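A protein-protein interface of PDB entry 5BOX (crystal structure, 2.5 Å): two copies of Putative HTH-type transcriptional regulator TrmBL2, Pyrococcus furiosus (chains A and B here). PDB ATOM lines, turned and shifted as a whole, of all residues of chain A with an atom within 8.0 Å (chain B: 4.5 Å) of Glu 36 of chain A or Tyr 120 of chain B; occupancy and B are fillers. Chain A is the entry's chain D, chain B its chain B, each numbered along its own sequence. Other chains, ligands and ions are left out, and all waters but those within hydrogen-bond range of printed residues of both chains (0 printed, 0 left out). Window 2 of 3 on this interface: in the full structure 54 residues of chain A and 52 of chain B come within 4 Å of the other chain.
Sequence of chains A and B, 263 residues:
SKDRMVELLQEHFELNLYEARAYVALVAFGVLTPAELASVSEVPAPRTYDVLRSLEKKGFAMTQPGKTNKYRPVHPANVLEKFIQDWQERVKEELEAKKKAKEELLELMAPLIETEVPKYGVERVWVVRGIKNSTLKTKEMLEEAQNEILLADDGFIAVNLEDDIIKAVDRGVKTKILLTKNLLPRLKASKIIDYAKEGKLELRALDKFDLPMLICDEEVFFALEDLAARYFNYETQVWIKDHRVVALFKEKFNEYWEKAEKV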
ATOM      1  N   ALA A  25      11.257   8.060   1.228  1.00  0.00           N
ATOM      2  CA  ALA A  25      10.794   6.839   0.588  1.00  0.00           C
ATOM      3  C   ALA A  25      11.960   5.859   0.454  1.00  0.00           C
ATOM      4  O   ALA A  25      11.830   4.672   0.765  1.00  0.00           O
ATOM      5  CB  ALA A  25      10.179   7.143  -0.770  1.00  0.00           C
ATOM      6  N   PHE A  29      11.812   2.161   2.263  1.00  0.00           N
ATOM      7  CA  PHE A  29      11.690   0.899   1.545  1.00  0.00           C
ATOM      8  C   PHE A  29      13.039   0.285   1.198  1.00  0.00           C
ATOM      9  O   PHE A  29      13.097  -0.751   0.538  1.00  0.00           O
ATOM     10  CB  PHE A  29      10.866   1.088   0.271  1.00  0.00           C
ATOM     11  CG  PHE A  29       9.471   1.571   0.523  1.00  0.00           C
ATOM     12  CD1 PHE A  29       8.471   0.679   0.877  1.00  0.00           C
ATOM     13  CD2 PHE A  29       9.154   2.914   0.391  1.00  0.00           C
ATOM     14  CE1 PHE A  29       7.183   1.118   1.109  1.00  0.00           C
ATOM     15  CE2 PHE A  29       7.867   3.361   0.616  1.00  0.00           C
ATOM     16  CZ  PHE A  29       6.878   2.462   0.976  1.00  0.00           C
ATOM     17  N   VAL A  31      15.102   0.105  -0.950  1.00  0.00           N
ATOM     18  CA  VAL A  31      15.438   0.122  -2.369  1.00  0.00           C
ATOM     19  C   VAL A  31      14.198   0.513  -3.155  1.00  0.00           C
ATOM     20  O   VAL A  31      13.092   0.107  -2.805  1.00  0.00           O
ATOM     21  CB  VAL A  31      15.970  -1.243  -2.854  1.00  0.00           C
ATOM     22  CG1 VAL A  31      16.315  -1.185  -4.338  1.00  0.00           C
ATOM     23  CG2 VAL A  31      17.174  -1.676  -2.035  1.00  0.00           C
ATOM     24  N   LEU A  32      14.372   1.295  -4.216  1.00  0.00           N
ATOM     25  CA  LEU A  32      13.240   1.689  -5.052  1.00  0.00           C
ATOM     26  C   LEU A  32      13.628   1.962  -6.495  1.00  0.00           C
ATOM     27  O   LEU A  32      14.621   2.642  -6.774  1.00  0.00           O
ATOM     28  CB  LEU A  32      12.553   2.929  -4.488  1.00  0.00           C
ATOM     29  CG  LEU A  32      11.739   2.796  -3.209  1.00  0.00           C
ATOM     30  CD1 LEU A  32      11.385   4.187  -2.706  1.00  0.00           C
ATOM     31  CD2 LEU A  32      10.484   1.980  -3.479  1.00  0.00           C
ATOM     32  N   THR A  33      12.823   1.427  -7.404  1.00  0.00           N
ATOM     33  CA  THR A  33      12.896   1.783  -8.807  1.00  0.00           C
ATOM     34  C   THR A  33      12.058   3.046  -8.980  1.00  0.00           C
ATOM     35  O   THR A  33      11.185   3.320  -8.154  1.00  0.00           O
ATOM     36  CB  THR A  33      12.372   0.653  -9.702  1.00  0.00           C
ATOM     37  OG1 THR A  33      12.782   0.875 -11.055  1.00  0.00           O
ATOM     38  CG2 THR A  33      10.861   0.598  -9.646  1.00  0.00           C
ATOM     39  N   PRO A  34      12.323   3.824 -10.042  1.00  0.00           N
ATOM     40  CA  PRO A  34      11.559   5.054 -10.279  1.00  0.00           C
ATOM     41  C   PRO A  34      10.046   4.835 -10.254  1.00  0.00           C
ATOM     42  O   PRO A  34       9.326   5.631  -9.657  1.00  0.00           O
ATOM     43  CB  PRO A  34      12.029   5.494 -11.667  1.00  0.00           C
ATOM     44  CG  PRO A  34      13.408   4.933 -11.781  1.00  0.00           C
ATOM     45  CD  PRO A  34      13.382   3.625 -11.045  1.00  0.00           C
ATOM     46  N   ALA A  35       9.583   3.762 -10.888  1.00  0.00           N
ATOM     47  CA  ALA A  35       8.161   3.423 -10.903  1.00  0.00           C
ATOM     48  C   ALA A  35       7.668   3.132  -9.489  1.00  0.00           C
ATOM     49  O   ALA A  35       6.620   3.619  -9.073  1.00  0.00           O
ATOM     50  CB  ALA A  35       7.907   2.245 -11.808  1.00  0.00           C
ATOM     51  N   GLU A  36       8.410   2.309  -8.762  1.00  0.00           N
ATOM     52  CA  GLU A  36       8.045   1.985  -7.390  1.00  0.00           C
ATOM     53  C   GLU A  36       7.878   3.244  -6.548  1.00  0.00           C
ATOM     54  O   GLU A  36       6.943   3.342  -5.759  1.00  0.00           O
ATOM     55  CB  GLU A  36       9.080   1.048  -6.759  1.00  0.00           C
ATOM     56  CG  GLU A  36       8.992  -0.357  -7.317  1.00  0.00           C
ATOM     57  CD  GLU A  36      10.015  -1.301  -6.735  1.00  0.00           C
ATOM     58  OE1 GLU A  36      11.095  -0.832  -6.312  1.00  0.00           O
ATOM     59  OE2 GLU A  36       9.724  -2.519  -6.687  1.00  0.00           O
ATOM     60  N   LEU A  37       8.789   4.200  -6.720  1.00  0.00           N
ATOM     61  CA  LEU A  37       8.710   5.484  -6.026  1.00  0.00           C
ATOM     62  C   LEU A  37       7.432   6.237  -6.397  1.00  0.00           C
ATOM     63  O   LEU A  37       6.734   6.763  -5.528  1.00  0.00           O
ATOM     64  CB  LEU A  37       9.941   6.334  -6.348  1.00  0.00           C
ATOM     65  CG  LEU A  37      10.006   7.781  -5.848  1.00  0.00           C
ATOM     66  CD1 LEU A  37       9.993   7.872  -4.320  1.00  0.00           C
ATOM     67  CD2 LEU A  37      11.247   8.438  -6.412  1.00  0.00           C
ATOM     68  N   ALA A  38       7.124   6.281  -7.688  1.00  0.00           N
ATOM     69  CA  ALA A  38       5.931   6.972  -8.152  1.00  0.00           C
ATOM     70  C   ALA A  38       4.680   6.377  -7.501  1.00  0.00           C
ATOM     71  O   ALA A  38       3.704   7.084  -7.248  1.00  0.00           O
ATOM     72  CB  ALA A  38       5.835   6.906  -9.674  1.00  0.00           C
ATOM     73  N   SER A  39       4.729   5.081  -7.207  1.00  0.00           N
ATOM     74  CA  SER A  39       3.584   4.377  -6.640  1.00  0.00           C
ATOM     75  C   SER A  39       3.359   4.693  -5.160  1.00  0.00           C
ATOM     76  O   SER A  39       2.310   5.216  -4.782  1.00  0.00           O
ATOM     77  CB  SER A  39       3.761   2.868  -6.811  1.00  0.00           C
ATOM     78  OG  SER A  39       3.850   2.517  -8.181  1.00  0.00           O
ATOM     79  N   VAL A  40       4.350   4.378  -4.332  1.00  0.00           N
ATOM     80  CA  VAL A  40       4.207   4.478  -2.884  1.00  0.00           C
ATOM     81  C   VAL A  40       4.246   5.917  -2.380  1.00  0.00           C
ATOM     82  O   VAL A  40       3.841   6.181  -1.251  1.00  0.00           O
ATOM     83  CB  VAL A  40       5.302   3.661  -2.158  1.00  0.00           C
ATOM     84  CG1 VAL A  40       5.333   2.223  -2.660  1.00  0.00           C
ATOM     85  CG2 VAL A  40       6.667   4.332  -2.303  1.00  0.00           C
ATOM     86  N   SER A  41       4.757   6.842  -3.193  1.00  0.00           N
ATOM     87  CA  SER A  41       4.980   8.211  -2.723  1.00  0.00           C
ATOM     88  C   SER A  41       4.200   9.239  -3.531  1.00  0.00           C
ATOM     89  O   SER A  41       3.546   8.900  -4.517  1.00  0.00           O
ATOM     90  CB  SER A  41       6.469   8.557  -2.761  1.00  0.00           C
ATOM     91  OG  SER A  41       6.934   8.664  -4.095  1.00  0.00           O
ATOM     92  N   VAL A  43       5.504  11.686  -5.196  1.00  0.00           N
ATOM     93  CA  VAL A  43       6.355  12.239  -6.238  1.00  0.00           C
ATOM     94  C   VAL A  43       5.825  11.812  -7.604  1.00  0.00           C
ATOM     95  O   VAL A  43       5.739  10.619  -7.897  1.00  0.00           O
ATOM     96  CB  VAL A  43       7.820  11.817  -6.053  1.00  0.00           C
ATOM     97  CG1 VAL A  43       8.690  12.410  -7.156  1.00  0.00           C
ATOM     98  CG2 VAL A  43       8.318  12.259  -4.686  1.00  0.00           C
ATOM     99  N   THR A  48      10.103  11.132 -11.062  1.00  0.00           N
ATOM    100  CA  THR A  48      10.871  10.220 -10.223  1.00  0.00           C
ATOM    101  C   THR A  48      12.315  10.067 -10.703  1.00  0.00           C
ATOM    102  O   THR A  48      13.234   9.983  -9.887  1.00  0.00           O
ATOM    103  CB  THR A  48      10.205   8.827 -10.153  1.00  0.00           C
ATOM    104  OG1 THR A  48       9.891   8.370 -11.474  1.00  0.00           O
ATOM    105  CG2 THR A  48       8.940   8.871  -9.304  1.00  0.00           C
ATOM    106  N   LEU A  52      15.381  11.227  -8.565  1.00  0.00           N
ATOM    107  CA  LEU A  52      16.298  10.219  -8.052  1.00  0.00           C
ATOM    108  C   LEU A  52      17.734  10.494  -8.491  1.00  0.00           C
ATOM    109  O   LEU A  52      18.662  10.393  -7.688  1.00  0.00           O
ATOM    110  CB  LEU A  52      15.849   8.825  -8.490  1.00  0.00           C
ATOM    111  CG  LEU A  52      14.713   8.248  -7.640  1.00  0.00           C
ATOM    112  CD1 LEU A  52      14.112   7.027  -8.299  1.00  0.00           C
ATOM    113  CD2 LEU A  52      15.230   7.890  -6.251  1.00  0.00           C
ATOM    114  N   ASN A  69      18.536   0.588 -12.401  1.00  0.00           N
ATOM    115  CA  ASN A  69      17.126   0.961 -12.378  1.00  0.00           C
ATOM    116  C   ASN A  69      16.675   1.117 -10.932  1.00  0.00           C
ATOM    117  O   ASN A  69      15.599   1.638 -10.660  1.00  0.00           O
ATOM    118  CB  ASN A  69      16.262  -0.084 -13.089  1.00  0.00           C
ATOM    119  CG  ASN A  69      16.543  -0.164 -14.574  1.00  0.00           C
ATOM    120  OD1 ASN A  69      16.726  -1.251 -15.127  1.00  0.00           O
ATOM    121  ND2 ASN A  69      16.575   0.990 -15.231  1.00  0.00           N
ATOM    122  N   LYS A  70      17.516   0.658 -10.008  1.00  0.00           N
ATOM    123  CA  LYS A  70      17.195   0.670  -8.584  1.00  0.00           C
ATOM    124  C   LYS A  70      18.051   1.648  -7.791  1.00  0.00           C
ATOM    125  O   LYS A  70      19.265   1.730  -7.991  1.00  0.00           O
ATOM    126  CB  LYS A  70      17.377  -0.730  -7.995  1.00  0.00           C
ATOM    127  CG  LYS A  70      16.713  -1.848  -8.781  1.00  0.00           C
ATOM    128  CD  LYS A  70      16.598  -3.103  -7.929  1.00  0.00           C
ATOM    129  CE  LYS A  70      16.184  -4.309  -8.754  1.00  0.00           C
ATOM    130  NZ  LYS A  70      16.746  -5.569  -8.190  1.00  0.00           N
ATOM    131  N   TYR A  71      17.419   2.367  -6.868  1.00  0.00           N
ATOM    132  CA  TYR A  71      18.133   3.321  -6.030  1.00  0.00           C
ATOM    133  C   TYR A  71      18.009   2.944  -4.561  1.00  0.00           C
ATOM    134  O   TYR A  71      16.930   2.583  -4.087  1.00  0.00           O
ATOM    135  CB  TYR A  71      17.605   4.741  -6.233  1.00  0.00           C
ATOM    136  CG  TYR A  71      17.997   5.386  -7.538  1.00  0.00           C
ATOM    137  CD1 TYR A  71      17.319   5.084  -8.710  1.00  0.00           C
ATOM    138  CD2 TYR A  71      19.027   6.313  -7.598  1.00  0.00           C
ATOM    139  CE1 TYR A  71      17.659   5.675  -9.904  1.00  0.00           C
ATOM    140  CE2 TYR A  71      19.376   6.912  -8.792  1.00  0.00           C
ATOM    141  CZ  TYR A  71      18.687   6.589  -9.942  1.00  0.00           C
ATOM    142  OH  TYR A  71      19.025   7.179 -11.137  1.00  0.00           O
ATOM    143  N   PRO B 118      14.299  -5.561  -0.441  1.00  0.00           N
ATOM    144  CA  PRO B 118      13.169  -6.068  -1.228  1.00  0.00           C
ATOM    145  C   PRO B 118      13.616  -6.646  -2.566  1.00  0.00           C
ATOM    146  O   PRO B 118      14.388  -6.005  -3.282  1.00  0.00           O
ATOM    147  CB  PRO B 118      12.300  -4.824  -1.433  1.00  0.00           C
ATOM    148  CG  PRO B 118      13.257  -3.678  -1.326  1.00  0.00           C
ATOM    149  CD  PRO B 118      14.261  -4.096  -0.294  1.00  0.00           C
ATOM    150  N   LYS B 119      13.142  -7.846  -2.891  1.00  0.00           N
ATOM    151  CA  LYS B 119      13.512  -8.500  -4.142  1.00  0.00           C
ATOM    152  C   LYS B 119      12.436  -8.399  -5.224  1.00  0.00           C
ATOM    153  O   LYS B 119      12.634  -8.884  -6.338  1.00  0.00           O
ATOM    154  CB  LYS B 119      13.844  -9.972  -3.890  1.00  0.00           C
ATOM    155  CG  LYS B 119      15.207 -10.210  -3.254  1.00  0.00           C
ATOM    156  CD  LYS B 119      16.337  -9.750  -4.171  1.00  0.00           C
ATOM    157  CE  LYS B 119      17.707 -10.048  -3.573  1.00  0.00           C
ATOM    158  NZ  LYS B 119      17.932  -9.374  -2.264  1.00  0.00           N
ATOM    159  N   TYR B 120      11.301  -7.784  -4.905  1.00  0.00           N
ATOM    160  CA  TYR B 120      10.222  -7.668  -5.887  1.00  0.00           C
ATOM    161  C   TYR B 120       9.761  -6.241  -6.253  1.00  0.00           C
ATOM    162  O   TYR B 120       9.447  -5.995  -7.417  1.00  0.00           O
ATOM    163  CB  TYR B 120       9.020  -8.493  -5.416  1.00  0.00           C
ATOM    164  CG  TYR B 120       9.262  -9.988  -5.523  1.00  0.00           C
ATOM    165  CD1 TYR B 120      10.165 -10.498  -6.447  1.00  0.00           C
ATOM    166  CD2 TYR B 120       8.594 -10.883  -4.701  1.00  0.00           C
ATOM    167  CE1 TYR B 120      10.396 -11.859  -6.550  1.00  0.00           C
ATOM    168  CE2 TYR B 120       8.817 -12.248  -4.798  1.00  0.00           C
ATOM    169  CZ  TYR B 120       9.719 -12.729  -5.724  1.00  0.00           C
ATOM    170  OH  TYR B 120       9.945 -14.082  -5.823  1.00  0.00           O
ATOM    171  N   GLY B 121       9.701  -5.305  -5.305  1.00  0.00           N
ATOM    172  CA  GLY B 121       9.995  -5.533  -3.904  1.00  0.00           C
ATOM    173  C   GLY B 121       8.953  -4.913  -2.993  1.00  0.00           C
ATOM    174  O   GLY B 121       8.800  -5.326  -1.845  1.00  0.00           O
ATOM    175  N   VAL B 122       8.241  -3.910  -3.494  1.00  0.00           N
ATOM    176  CA  VAL B 122       7.188  -3.284  -2.706  1.00  0.00           C
ATOM    177  C   VAL B 122       5.951  -4.175  -2.718  1.00  0.00           C
ATOM    178  O   VAL B 122       5.045  -4.020  -1.899  1.00  0.00           O
ATOM    179  CB  VAL B 122       6.860  -1.876  -3.227  1.00  0.00           C
ATOM    180  CG1 VAL B 122       8.123  -1.039  -3.306  1.00  0.00           C
ATOM    181  CG2 VAL B 122       6.176  -1.952  -4.585  1.00  0.00           C
ATOM    182  N   GLU B 123       5.937  -5.123  -3.649  1.00  0.00           N
ATOM    183  CA  GLU B 123       4.827  -6.055  -3.803  1.00  0.00           C
ATOM    184  C   GLU B 123       4.905  -7.186  -2.793  1.00  0.00           C
ATOM    185  O   GLU B 123       5.919  -7.871  -2.701  1.00  0.00           O
ATOM    186  CB  GLU B 123       4.804  -6.638  -5.216  1.00  0.00           C
ATOM    187  CG  GLU B 123       4.252  -5.708  -6.273  1.00  0.00           C
ATOM    188  CD  GLU B 123       2.796  -5.372  -6.034  1.00  0.00           C
ATOM    189  OE1 GLU B 123       2.213  -5.893  -5.052  1.00  0.00           O
ATOM    190  OE2 GLU B 123       2.235  -4.596  -6.834  1.00  0.00           O
ATOM    191  N   LYS B 137       7.220 -19.077 -10.320  1.00  0.00           N
ATOM    192  CA  LYS B 137       7.066 -18.456  -9.008  1.00  0.00           C
ATOM    193  C   LYS B 137       7.487 -19.398  -7.890  1.00  0.00           C
ATOM    194  O   LYS B 137       8.080 -18.972  -6.899  1.00  0.00           O
ATOM    195  CB  LYS B 137       5.624 -17.998  -8.790  1.00  0.00           C
ATOM    196  CG  LYS B 137       5.458 -17.074  -7.599  1.00  0.00           C
ATOM    197  CD  LYS B 137       6.356 -15.854  -7.735  1.00  0.00           C
ATOM    198  CE  LYS B 137       6.323 -14.997  -6.478  1.00  0.00           C
ATOM    199  NZ  LYS B 137       6.925 -15.685  -5.308  1.00  0.00           N
ATOM    200  N   GLU B 140      11.287 -19.430  -7.812  1.00  0.00           N
ATOM    201  CA  GLU B 140      11.813 -18.286  -7.068  1.00  0.00           C
ATOM    202  C   GLU B 140      11.686 -18.486  -5.565  1.00  0.00           C
ATOM    203  O   GLU B 140      12.586 -18.130  -4.802  1.00  0.00           O
ATOM    204  CB  GLU B 140      11.093 -16.992  -7.462  1.00  0.00           C
ATOM    205  CG  GLU B 140      11.334 -16.526  -8.886  1.00  0.00           C
ATOM    206  CD  GLU B 140      10.678 -15.184  -9.178  1.00  0.00           C
ATOM    207  OE1 GLU B 140      10.781 -14.266  -8.334  1.00  0.00           O
ATOM    208  OE2 GLU B 140      10.059 -15.049 -10.254  1.00  0.00           O
ATOM    209  N   GLU B 144      14.955 -18.588  -3.126  1.00  0.00           N
ATOM    210  CA  GLU B 144      15.143 -17.584  -2.087  1.00  0.00           C
ATOM    211  C   GLU B 144      14.956 -18.175  -0.697  1.00  0.00           C
ATOM    212  O   GLU B 144      15.076 -17.473   0.304  1.00  0.00           O
ATOM    213  CB  GLU B 144      14.183 -16.411  -2.296  1.00  0.00           C
ATOM    214  CG  GLU B 144      14.457 -15.595  -3.552  1.00  0.00           C
ATOM    215  CD  GLU B 144      13.450 -14.480  -3.755  1.00  0.00           C
ATOM    216  OE1 GLU B 144      12.370 -14.535  -3.129  1.00  0.00           O
ATOM    217  OE2 GLU B 144      13.744 -13.546  -4.533  1.00  0.00           O
ATOM    218  N   TRP B 239       0.225 -15.518  -4.302  1.00  0.00           N
ATOM    219  CA  TRP B 239       1.436 -15.465  -3.499  1.00  0.00           C
ATOM    220  C   TRP B 239       1.328 -14.313  -2.501  1.00  0.00           C
ATOM    221  O   TRP B 239       1.096 -13.170  -2.894  1.00  0.00           O
ATOM    222  CB  TRP B 239       2.658 -15.294  -4.413  1.00  0.00           C
ATOM    223  CG  TRP B 239       3.954 -15.039  -3.706  1.00  0.00           C
ATOM    224  CD1 TRP B 239       4.798 -15.974  -3.186  1.00  0.00           C
ATOM    225  CD2 TRP B 239       4.562 -13.767  -3.455  1.00  0.00           C
ATOM    226  NE1 TRP B 239       5.891 -15.364  -2.621  1.00  0.00           N
ATOM    227  CE2 TRP B 239       5.771 -14.009  -2.773  1.00  0.00           C
ATOM    228  CE3 TRP B 239       4.200 -12.444  -3.736  1.00  0.00           C
ATOM    229  CZ2 TRP B 239       6.618 -12.980  -2.369  1.00  0.00           C
ATOM    230  CZ3 TRP B 239       5.045 -11.425  -3.333  1.00  0.00           C
ATOM    231  CH2 TRP B 239       6.237 -11.699  -2.657  1.00  0.00           C
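Of the 19 printed residues of chain A, 4 touch a printed residue of chain B.
Along chain A the printed residues that touch a printed residue of chain B span positions 29 to 36.
Of the 10 printed residues of chain B, 4 touch a printed residue of chain A.
Printed residues of chain B that touch a printed residue of chain A: Pro 118, Tyr 120, Gly 121 and Val 122.
Hydrophobic or aromatic side chains of chain B within 4 Å of the printed part of chain A: Pro 118 and Val 122.
Among the printed residues, 6 pairs touch across the chains.
No position is printed for both chains.
Of the 6 pairs that touch across the chains among the printed residues, none has its exchanged pair printed and touching as well.
Of chain B, only Tyr 120, Gly 121 and Val 122 come within 4 Å of Glu 36 of chain A.
Tyr 120 of chain B touches just one residue of chain A: Glu 36 (3.6 Å).
Of the printed residues of chain A, Val 122 of chain B touches Leu 32 and Glu 36.
Of the printed residues of chain B, Val 31 of chain A touches Pro 118.
Printed residues of chain B within 4 Å of Phe 29 of chain A: Pro 118 (3.5 Å).
Asn 69 of chain A touches none of the printed residues of chain B.
Lys 119 of chain B touches none of the printed residues of chain A.
The nearest residue of chain A that does not touch Tyr 120 of chain B is Lys 70 of chain A (6.7 Å).
The backbone NH (N) of Gly 121 of chain B sits at hydrogen-bond distance from the side-chain carboxylate (OE2) of Glu 36 of chain A (3.1 Å).
Among the printed residues, merely in contact across the chains: Phe 29 of chain A with Pro 118 of chain B (3.5 Å), Glu 36 of chain A with Tyr 120 of chain B (3.6 Å), Glu 36 of chain A with Val 122 of chain B (3.8 Å), Leu 32 of chain A with Val 122 of chain B (3.8 Å) and Val 31 of chain A with Pro 118 of chain B (3.95 Å).
O of Leu 32 of chain A lies within hydrogen-bond range of N of Tyr 71 of chain A (2.8 Å).
The side-chain hydroxyl (OH) of Tyr 120 of chain B lies within hydrogen-bond range of the side-chain carboxylate (OE1) of Glu 140 of chain B (2.7 Å).
The side-chain amino group (NZ) of Lys 137 of chain B sits at hydrogen-bond distance from the side-chain hydroxyl (OH) of Tyr 120 of chain B, 3.5 Å away.
The backbone NH (N) of Thr 33 of chain A is in hydrogen-bond range of the side-chain carboxylate (OE1) of Glu 36 of chain A, 3.0 Å away.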
